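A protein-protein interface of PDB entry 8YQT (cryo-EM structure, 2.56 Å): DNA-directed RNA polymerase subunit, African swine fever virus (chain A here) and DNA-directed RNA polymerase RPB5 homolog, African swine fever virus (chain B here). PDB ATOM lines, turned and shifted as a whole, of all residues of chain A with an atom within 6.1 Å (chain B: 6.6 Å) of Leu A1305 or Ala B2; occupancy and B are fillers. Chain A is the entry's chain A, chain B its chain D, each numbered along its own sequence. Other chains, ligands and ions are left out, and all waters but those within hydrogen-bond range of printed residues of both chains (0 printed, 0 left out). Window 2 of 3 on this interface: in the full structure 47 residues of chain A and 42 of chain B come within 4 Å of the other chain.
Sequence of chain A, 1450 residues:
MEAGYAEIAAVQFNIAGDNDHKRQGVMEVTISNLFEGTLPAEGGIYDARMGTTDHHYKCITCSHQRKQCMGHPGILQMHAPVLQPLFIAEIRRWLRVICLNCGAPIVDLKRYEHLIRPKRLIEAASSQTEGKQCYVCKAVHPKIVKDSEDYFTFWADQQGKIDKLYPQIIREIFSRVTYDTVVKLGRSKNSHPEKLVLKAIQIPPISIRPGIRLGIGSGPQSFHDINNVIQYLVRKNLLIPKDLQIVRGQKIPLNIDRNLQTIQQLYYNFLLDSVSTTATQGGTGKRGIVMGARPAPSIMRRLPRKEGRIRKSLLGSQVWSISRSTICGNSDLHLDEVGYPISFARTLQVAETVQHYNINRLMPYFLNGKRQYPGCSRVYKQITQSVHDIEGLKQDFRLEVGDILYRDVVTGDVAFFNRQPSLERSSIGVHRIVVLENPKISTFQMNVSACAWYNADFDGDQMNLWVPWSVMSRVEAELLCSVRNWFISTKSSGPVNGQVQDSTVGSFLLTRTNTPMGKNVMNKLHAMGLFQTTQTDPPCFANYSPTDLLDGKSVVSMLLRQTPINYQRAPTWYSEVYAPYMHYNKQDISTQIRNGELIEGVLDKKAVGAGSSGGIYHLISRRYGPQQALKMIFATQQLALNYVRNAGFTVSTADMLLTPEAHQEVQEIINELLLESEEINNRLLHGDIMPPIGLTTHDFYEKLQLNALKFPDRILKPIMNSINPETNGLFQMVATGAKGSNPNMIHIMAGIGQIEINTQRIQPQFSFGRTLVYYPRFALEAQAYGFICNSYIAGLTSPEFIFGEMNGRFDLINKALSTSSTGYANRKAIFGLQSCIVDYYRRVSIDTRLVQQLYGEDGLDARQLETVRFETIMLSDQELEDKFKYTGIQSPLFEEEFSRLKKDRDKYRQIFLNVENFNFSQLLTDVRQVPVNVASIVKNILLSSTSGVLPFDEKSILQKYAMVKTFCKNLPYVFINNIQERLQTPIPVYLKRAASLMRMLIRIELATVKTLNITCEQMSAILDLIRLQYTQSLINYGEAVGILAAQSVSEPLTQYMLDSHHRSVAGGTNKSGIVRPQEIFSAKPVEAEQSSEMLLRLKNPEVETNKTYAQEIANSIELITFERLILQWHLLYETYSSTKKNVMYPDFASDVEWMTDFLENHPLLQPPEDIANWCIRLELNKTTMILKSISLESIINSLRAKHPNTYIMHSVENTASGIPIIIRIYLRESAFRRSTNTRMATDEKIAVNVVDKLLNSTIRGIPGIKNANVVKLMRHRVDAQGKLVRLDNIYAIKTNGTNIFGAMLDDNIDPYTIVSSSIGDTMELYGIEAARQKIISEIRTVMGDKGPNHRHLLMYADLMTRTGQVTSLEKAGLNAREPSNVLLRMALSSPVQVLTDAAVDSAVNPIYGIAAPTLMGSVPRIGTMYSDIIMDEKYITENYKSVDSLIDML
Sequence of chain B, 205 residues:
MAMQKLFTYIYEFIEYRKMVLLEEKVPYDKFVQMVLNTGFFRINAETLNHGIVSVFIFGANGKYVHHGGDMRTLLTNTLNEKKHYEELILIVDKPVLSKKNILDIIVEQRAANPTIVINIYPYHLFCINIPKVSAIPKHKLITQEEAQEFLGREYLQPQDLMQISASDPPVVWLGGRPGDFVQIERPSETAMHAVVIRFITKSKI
Among the printed residues, pairs that only touch across the chains: Phe A1301 with His B124, Phe A1301 with Cys B127, Leu A1305 with Ala B2 and Leu A1305 with Lys B5.
The backbone carbonyl oxygen (O) of Tyr B123 sits at hydrogen-bond distance from the side-chain sulfur (SG) of Cys B127, 3.4 Å away.
OD1 of Asp A1307 is in salt-bridge range of NZ of Lys B5.
O of Leu A1305 sits close to SD of Met B1.
OD2 of Asp A1307 lies close to SD of Met B1 (3.5 Å).
Hydrophobic or aromatic side chains of chain A that line the printed part of chain B: Phe A1301 and Leu A1305.
Of the 12 printed residues of chain B, 5 touch a printed residue of chain A.
Among the printed residues, Asp or Glu carboxylates within 4 Å of a Lys or Arg side-chain nitrogen of the other chain: Asp A1307 with Lys B5 (2.8 Å).
Of chain A, only Leu A1305 comes within 4 Å of Ala B2.
Printed residues of chain A within 4 Å of His B124: Phe A1301 (3.5 Å).
Of the printed residues of chain A, Lys B5 touches Leu A1305 and Asp A1307.
Printed residues of chain A within 4 Å of Cys B127: Phe A1301 (3.5 Å).
Ala A1303 touches none of the printed residues of chain B.
Phe B7 touches none of the printed residues of chain A.
The nearest residue of chain A that does not touch Ala B2 is Phe A1301 (4.2 Å).
The nearest printed residue of chain A that does not touch Cys B127 is Met A1304 (4.2 Å).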
ATOM      1  N   ILE A1300     -17.572 -18.752  -3.515  1.00  0.00           N
ATOM      2  CA  ILE A1300     -16.325 -18.744  -2.758  1.00  0.00           C
ATOM      3  C   ILE A1300     -16.451 -19.616  -1.519  1.00  0.00           C
ATOM      4  O   ILE A1300     -15.539 -20.378  -1.186  1.00  0.00           O
ATOM      5  CB  ILE A1300     -15.920 -17.302  -2.400  1.00  0.00           C
ATOM      6  CG1 ILE A1300     -15.658 -16.487  -3.664  1.00  0.00           C
ATOM      7  CG2 ILE A1300     -14.693 -17.294  -1.504  1.00  0.00           C
ATOM      8  CD1 ILE A1300     -15.282 -15.056  -3.389  1.00  0.00           C
ATOM      9  N   PHE A1301     -17.580 -19.519  -0.818  1.00  0.00           N
ATOM     10  CA  PHE A1301     -17.784 -20.324   0.379  1.00  0.00           C
ATOM     11  C   PHE A1301     -17.862 -21.810   0.046  1.00  0.00           C
ATOM     12  O   PHE A1301     -17.331 -22.646   0.788  1.00  0.00           O
ATOM     13  CB  PHE A1301     -19.048 -19.861   1.101  1.00  0.00           C
ATOM     14  CG  PHE A1301     -19.155 -20.352   2.511  1.00  0.00           C
ATOM     15  CD1 PHE A1301     -20.391 -20.580   3.084  1.00  0.00           C
ATOM     16  CD2 PHE A1301     -18.020 -20.583   3.263  1.00  0.00           C
ATOM     17  CE1 PHE A1301     -20.494 -21.027   4.381  1.00  0.00           C
ATOM     18  CE2 PHE A1301     -18.117 -21.031   4.558  1.00  0.00           C
ATOM     19  CZ  PHE A1301     -19.358 -21.253   5.119  1.00  0.00           C
ATOM     20  N   GLY A1302     -18.521 -22.160  -1.061  1.00  0.00           N
ATOM     21  CA  GLY A1302     -18.605 -23.559  -1.449  1.00  0.00           C
ATOM     22  C   GLY A1302     -17.261 -24.150  -1.830  1.00  0.00           C
ATOM     23  O   GLY A1302     -16.923 -25.260  -1.412  1.00  0.00           O
ATOM     24  N   ALA A1303     -16.479 -23.422  -2.632  1.00  0.00           N
ATOM     25  CA  ALA A1303     -15.122 -23.848  -2.955  1.00  0.00           C
ATOM     26  C   ALA A1303     -14.227 -23.889  -1.727  1.00  0.00           C
ATOM     27  O   ALA A1303     -13.365 -24.766  -1.625  1.00  0.00           O
ATOM     28  CB  ALA A1303     -14.518 -22.920  -4.007  1.00  0.00           C
ATOM     29  N   MET A1304     -14.420 -22.959  -0.798  1.00  0.00           N
ATOM     30  CA  MET A1304     -13.702 -22.932   0.467  1.00  0.00           C
ATOM     31  C   MET A1304     -13.944 -24.163   1.323  1.00  0.00           C
ATOM     32  O   MET A1304     -13.024 -24.610   2.015  1.00  0.00           O
ATOM     33  CB  MET A1304     -14.127 -21.693   1.237  1.00  0.00           C
ATOM     34  CG  MET A1304     -13.459 -21.474   2.550  1.00  0.00           C
ATOM     35  SD  MET A1304     -14.299 -20.072   3.278  1.00  0.00           S
ATOM     36  CE  MET A1304     -14.516 -19.051   1.828  1.00  0.00           C
ATOM     37  N   LEU A1305     -15.157 -24.711   1.306  1.00  0.00           N
ATOM     38  CA  LEU A1305     -15.471 -25.884   2.108  1.00  0.00           C
ATOM     39  C   LEU A1305     -14.895 -27.168   1.529  1.00  0.00           C
ATOM     40  O   LEU A1305     -14.913 -28.196   2.209  1.00  0.00           O
ATOM     41  CB  LEU A1305     -16.986 -26.018   2.264  1.00  0.00           C
ATOM     42  CG  LEU A1305     -17.684 -24.927   3.077  1.00  0.00           C
ATOM     43  CD1 LEU A1305     -19.191 -25.058   2.960  1.00  0.00           C
ATOM     44  CD2 LEU A1305     -17.255 -24.980   4.530  1.00  0.00           C
ATOM     45  N   ASP A1306     -14.387 -27.136   0.301  1.00  0.00           N
ATOM     46  CA  ASP A1306     -13.794 -28.318  -0.307  1.00  0.00           C
ATOM     47  C   ASP A1306     -12.366 -28.515   0.184  1.00  0.00           C
ATOM     48  O   ASP A1306     -11.586 -27.562   0.270  1.00  0.00           O
ATOM     49  CB  ASP A1306     -13.810 -28.196  -1.830  1.00  0.00           C
ATOM     50  CG  ASP A1306     -13.668 -29.534  -2.522  1.00  0.00           C
ATOM     51  OD1 ASP A1306     -13.732 -30.570  -1.830  1.00  0.00           O
ATOM     52  OD2 ASP A1306     -13.480 -29.552  -3.754  1.00  0.00           O
ATOM     53  N   ASP A1307     -12.023 -29.760   0.501  1.00  0.00           N
ATOM     54  CA  ASP A1307     -10.691 -30.101   0.981  1.00  0.00           C
ATOM     55  C   ASP A1307      -9.707 -30.378  -0.148  1.00  0.00           C
ATOM     56  O   ASP A1307      -8.529 -30.631   0.127  1.00  0.00           O
ATOM     57  CB  ASP A1307     -10.761 -31.309   1.915  1.00  0.00           C
ATOM     58  CG  ASP A1307     -11.221 -30.938   3.311  1.00  0.00           C
ATOM     59  OD1 ASP A1307     -10.816 -29.865   3.806  1.00  0.00           O
ATOM     60  OD2 ASP A1307     -11.992 -31.716   3.912  1.00  0.00           O
ATOM     61  N   MET B   1     -19.791 -28.178   4.756  1.00  0.00           N
ATOM     62  CA  MET B   1     -18.877 -28.760   5.728  1.00  0.00           C
ATOM     63  C   MET B   1     -18.528 -27.604   6.681  1.00  0.00           C
ATOM     64  O   MET B   1     -17.463 -27.537   7.290  1.00  0.00           O
ATOM     65  CB  MET B   1     -17.672 -29.404   5.000  1.00  0.00           C
ATOM     66  CG  MET B   1     -16.340 -29.549   5.738  1.00  0.00           C
ATOM     67  SD  MET B   1     -14.968 -30.015   4.668  1.00  0.00           S
ATOM     68  CE  MET B   1     -15.792 -31.098   3.501  1.00  0.00           C
ATOM     69  N   ALA B   2     -19.495 -26.696   6.827  1.00  0.00           N
ATOM     70  CA  ALA B   2     -19.272 -25.479   7.601  1.00  0.00           C
ATOM     71  C   ALA B   2     -18.956 -25.773   9.063  1.00  0.00           C
ATOM     72  O   ALA B   2     -18.158 -25.057   9.671  1.00  0.00           O
ATOM     73  CB  ALA B   2     -20.487 -24.560   7.495  1.00  0.00           C
ATOM     74  N   MET B   3     -19.565 -26.807   9.644  1.00  0.00           N
ATOM     75  CA  MET B   3     -19.293 -27.128  11.041  1.00  0.00           C
ATOM     76  C   MET B   3     -17.842 -27.545  11.249  1.00  0.00           C
ATOM     77  O   MET B   3     -17.211 -27.148  12.237  1.00  0.00           O
ATOM     78  CB  MET B   3     -20.238 -28.226  11.522  1.00  0.00           C
ATOM     79  CG  MET B   3     -21.701 -27.844  11.459  1.00  0.00           C
ATOM     80  SD  MET B   3     -22.166 -26.767  12.825  1.00  0.00           S
ATOM     81  CE  MET B   3     -22.581 -25.272  11.935  1.00  0.00           C
ATOM     82  N   GLN B   4     -17.301 -28.354  10.335  1.00  0.00           N
ATOM     83  CA  GLN B   4     -15.920 -28.807  10.473  1.00  0.00           C
ATOM     84  C   GLN B   4     -14.946 -27.641  10.397  1.00  0.00           C
ATOM     85  O   GLN B   4     -13.994 -27.566  11.184  1.00  0.00           O
ATOM     86  CB  GLN B   4     -15.601 -29.846   9.399  1.00  0.00           C
ATOM     87  CG  GLN B   4     -14.164 -30.333   9.421  1.00  0.00           C
ATOM     88  CD  GLN B   4     -13.832 -31.120  10.672  1.00  0.00           C
ATOM     89  OE1 GLN B   4     -14.569 -32.025  11.061  1.00  0.00           O
ATOM     90  NE2 GLN B   4     -12.721 -30.779  11.310  1.00  0.00           N
ATOM     91  N   LYS B   5     -15.162 -26.721   9.456  1.00  0.00           N
ATOM     92  CA  LYS B   5     -14.307 -25.546   9.356  1.00  0.00           C
ATOM     93  C   LYS B   5     -14.457 -24.641  10.571  1.00  0.00           C
ATOM     94  O   LYS B   5     -13.461 -24.108  11.078  1.00  0.00           O
ATOM     95  CB  LYS B   5     -14.624 -24.774   8.076  1.00  0.00           C
ATOM     96  CG  LYS B   5     -14.533 -25.611   6.819  1.00  0.00           C
ATOM     97  CD  LYS B   5     -13.146 -26.192   6.648  1.00  0.00           C
ATOM     98  CE  LYS B   5     -13.047 -27.007   5.374  1.00  0.00           C
ATOM     99  NZ  LYS B   5     -11.722 -27.666   5.252  1.00  0.00           N
ATOM    100  N   LEU B   6     -15.695 -24.457  11.040  1.00  0.00           N
ATOM    101  CA  LEU B   6     -15.941 -23.614  12.201  1.00  0.00           C
ATOM    102  C   LEU B   6     -15.217 -24.145  13.427  1.00  0.00           C
ATOM    103  O   LEU B   6     -14.563 -23.383  14.142  1.00  0.00           O
ATOM    104  CB  LEU B   6     -17.440 -23.519  12.478  1.00  0.00           C
ATOM    105  CG  LEU B   6     -18.267 -22.516  11.673  1.00  0.00           C
ATOM    106  CD1 LEU B   6     -19.744 -22.780  11.880  1.00  0.00           C
ATOM    107  CD2 LEU B   6     -17.921 -21.098  12.073  1.00  0.00           C
ATOM    108  N   PHE B   7     -15.285 -25.458  13.661  1.00  0.00           N
ATOM    109  CA  PHE B   7     -14.715 -26.027  14.876  1.00  0.00           C
ATOM    110  C   PHE B   7     -13.222 -25.750  15.018  1.00  0.00           C
ATOM    111  O   PHE B   7     -12.704 -25.762  16.139  1.00  0.00           O
ATOM    112  CB  PHE B   7     -14.970 -27.532  14.912  1.00  0.00           C
ATOM    113  CG  PHE B   7     -14.484 -28.191  16.163  1.00  0.00           C
ATOM    114  CD1 PHE B   7     -15.130 -27.981  17.367  1.00  0.00           C
ATOM    115  CD2 PHE B   7     -13.370 -29.010  16.138  1.00  0.00           C
ATOM    116  CE1 PHE B   7     -14.678 -28.581  18.519  1.00  0.00           C
ATOM    117  CE2 PHE B   7     -12.914 -29.613  17.289  1.00  0.00           C
ATOM    118  CZ  PHE B   7     -13.568 -29.398  18.479  1.00  0.00           C
ATOM    119  N   TYR B  28     -14.521 -32.830  18.255  1.00  0.00           N
ATOM    120  CA  TYR B  28     -15.479 -32.366  17.257  1.00  0.00           C
ATOM    121  C   TYR B  28     -16.784 -33.153  17.294  1.00  0.00           C
ATOM    122  O   TYR B  28     -17.856 -32.577  17.073  1.00  0.00           O
ATOM    123  CB  TYR B  28     -14.848 -32.443  15.869  1.00  0.00           C
ATOM    124  CG  TYR B  28     -15.807 -32.201  14.729  1.00  0.00           C
ATOM    125  CD1 TYR B  28     -16.284 -30.928  14.457  1.00  0.00           C
ATOM    126  CD2 TYR B  28     -16.228 -33.245  13.918  1.00  0.00           C
ATOM    127  CE1 TYR B  28     -17.157 -30.701  13.413  1.00  0.00           C
ATOM    128  CE2 TYR B  28     -17.101 -33.029  12.873  1.00  0.00           C
ATOM    129  CZ  TYR B  28     -17.562 -31.755  12.624  1.00  0.00           C
ATOM    130  OH  TYR B  28     -18.433 -31.535  11.583  1.00  0.00           O
ATOM    131  N   TYR B 123     -21.797 -17.747   8.838  1.00  0.00           N
ATOM    132  CA  TYR B 123     -20.876 -18.861   9.030  1.00  0.00           C
ATOM    133  C   TYR B 123     -19.522 -18.590   8.391  1.00  0.00           C
ATOM    134  O   TYR B 123     -18.481 -18.851   9.001  1.00  0.00           O
ATOM    135  CB  TYR B 123     -21.478 -20.142   8.454  1.00  0.00           C
ATOM    136  CG  TYR B 123     -22.389 -20.875   9.402  1.00  0.00           C
ATOM    137  CD1 TYR B 123     -22.618 -20.398  10.684  1.00  0.00           C
ATOM    138  CD2 TYR B 123     -23.037 -22.036   9.011  1.00  0.00           C
ATOM    139  CE1 TYR B 123     -23.453 -21.063  11.551  1.00  0.00           C
ATOM    140  CE2 TYR B 123     -23.877 -22.705   9.869  1.00  0.00           C
ATOM    141  CZ  TYR B 123     -24.082 -22.214  11.138  1.00  0.00           C
ATOM    142  OH  TYR B 123     -24.918 -22.882  11.998  1.00  0.00           O
ATOM    143  N   HIS B 124     -19.516 -18.065   7.163  1.00  0.00           N
ATOM    144  CA  HIS B 124     -18.284 -17.981   6.390  1.00  0.00           C
ATOM    145  C   HIS B 124     -17.251 -17.050   7.003  1.00  0.00           C
ATOM    146  O   HIS B 124     -16.071 -17.158   6.660  1.00  0.00           O
ATOM    147  CB  HIS B 124     -18.579 -17.543   4.954  1.00  0.00           C
ATOM    148  CG  HIS B 124     -19.362 -16.274   4.851  1.00  0.00           C
ATOM    149  ND1 HIS B 124     -18.810 -15.037   5.103  1.00  0.00           N
ATOM    150  CD2 HIS B 124     -20.648 -16.047   4.495  1.00  0.00           C
ATOM    151  CE1 HIS B 124     -19.727 -14.104   4.921  1.00  0.00           C
ATOM    152  NE2 HIS B 124     -20.850 -14.690   4.550  1.00  0.00           N
ATOM    153  N   PHE B 126     -16.055 -17.195   9.877  1.00  0.00           N
ATOM    154  CA  PHE B 126     -15.196 -17.967  10.767  1.00  0.00           C
ATOM    155  C   PHE B 126     -14.836 -19.325  10.174  1.00  0.00           C
ATOM    156  O   PHE B 126     -14.474 -20.240  10.916  1.00  0.00           O
ATOM    157  CB  PHE B 126     -15.859 -18.153  12.133  1.00  0.00           C
ATOM    158  CG  PHE B 126     -16.178 -16.867  12.830  1.00  0.00           C
ATOM    159  CD1 PHE B 126     -15.221 -16.218  13.586  1.00  0.00           C
ATOM    160  CD2 PHE B 126     -17.435 -16.302  12.722  1.00  0.00           C
ATOM    161  CE1 PHE B 126     -15.514 -15.037  14.226  1.00  0.00           C
ATOM    162  CE2 PHE B 126     -17.730 -15.118  13.360  1.00  0.00           C
ATOM    163  CZ  PHE B 126     -16.769 -14.486  14.112  1.00  0.00           C
ATOM    164  N   CYS B 127     -14.941 -19.480   8.858  1.00  0.00           N
ATOM    165  CA  CYS B 127     -14.576 -20.719   8.187  1.00  0.00           C
ATOM    166  C   CYS B 127     -13.195 -20.664   7.546  1.00  0.00           C
ATOM    167  O   CYS B 127     -12.795 -21.629   6.890  1.00  0.00           O
ATOM    168  CB  CYS B 127     -15.629 -21.075   7.132  1.00  0.00           C
ATOM    169  SG  CYS B 127     -17.161 -21.749   7.817  1.00  0.00           S
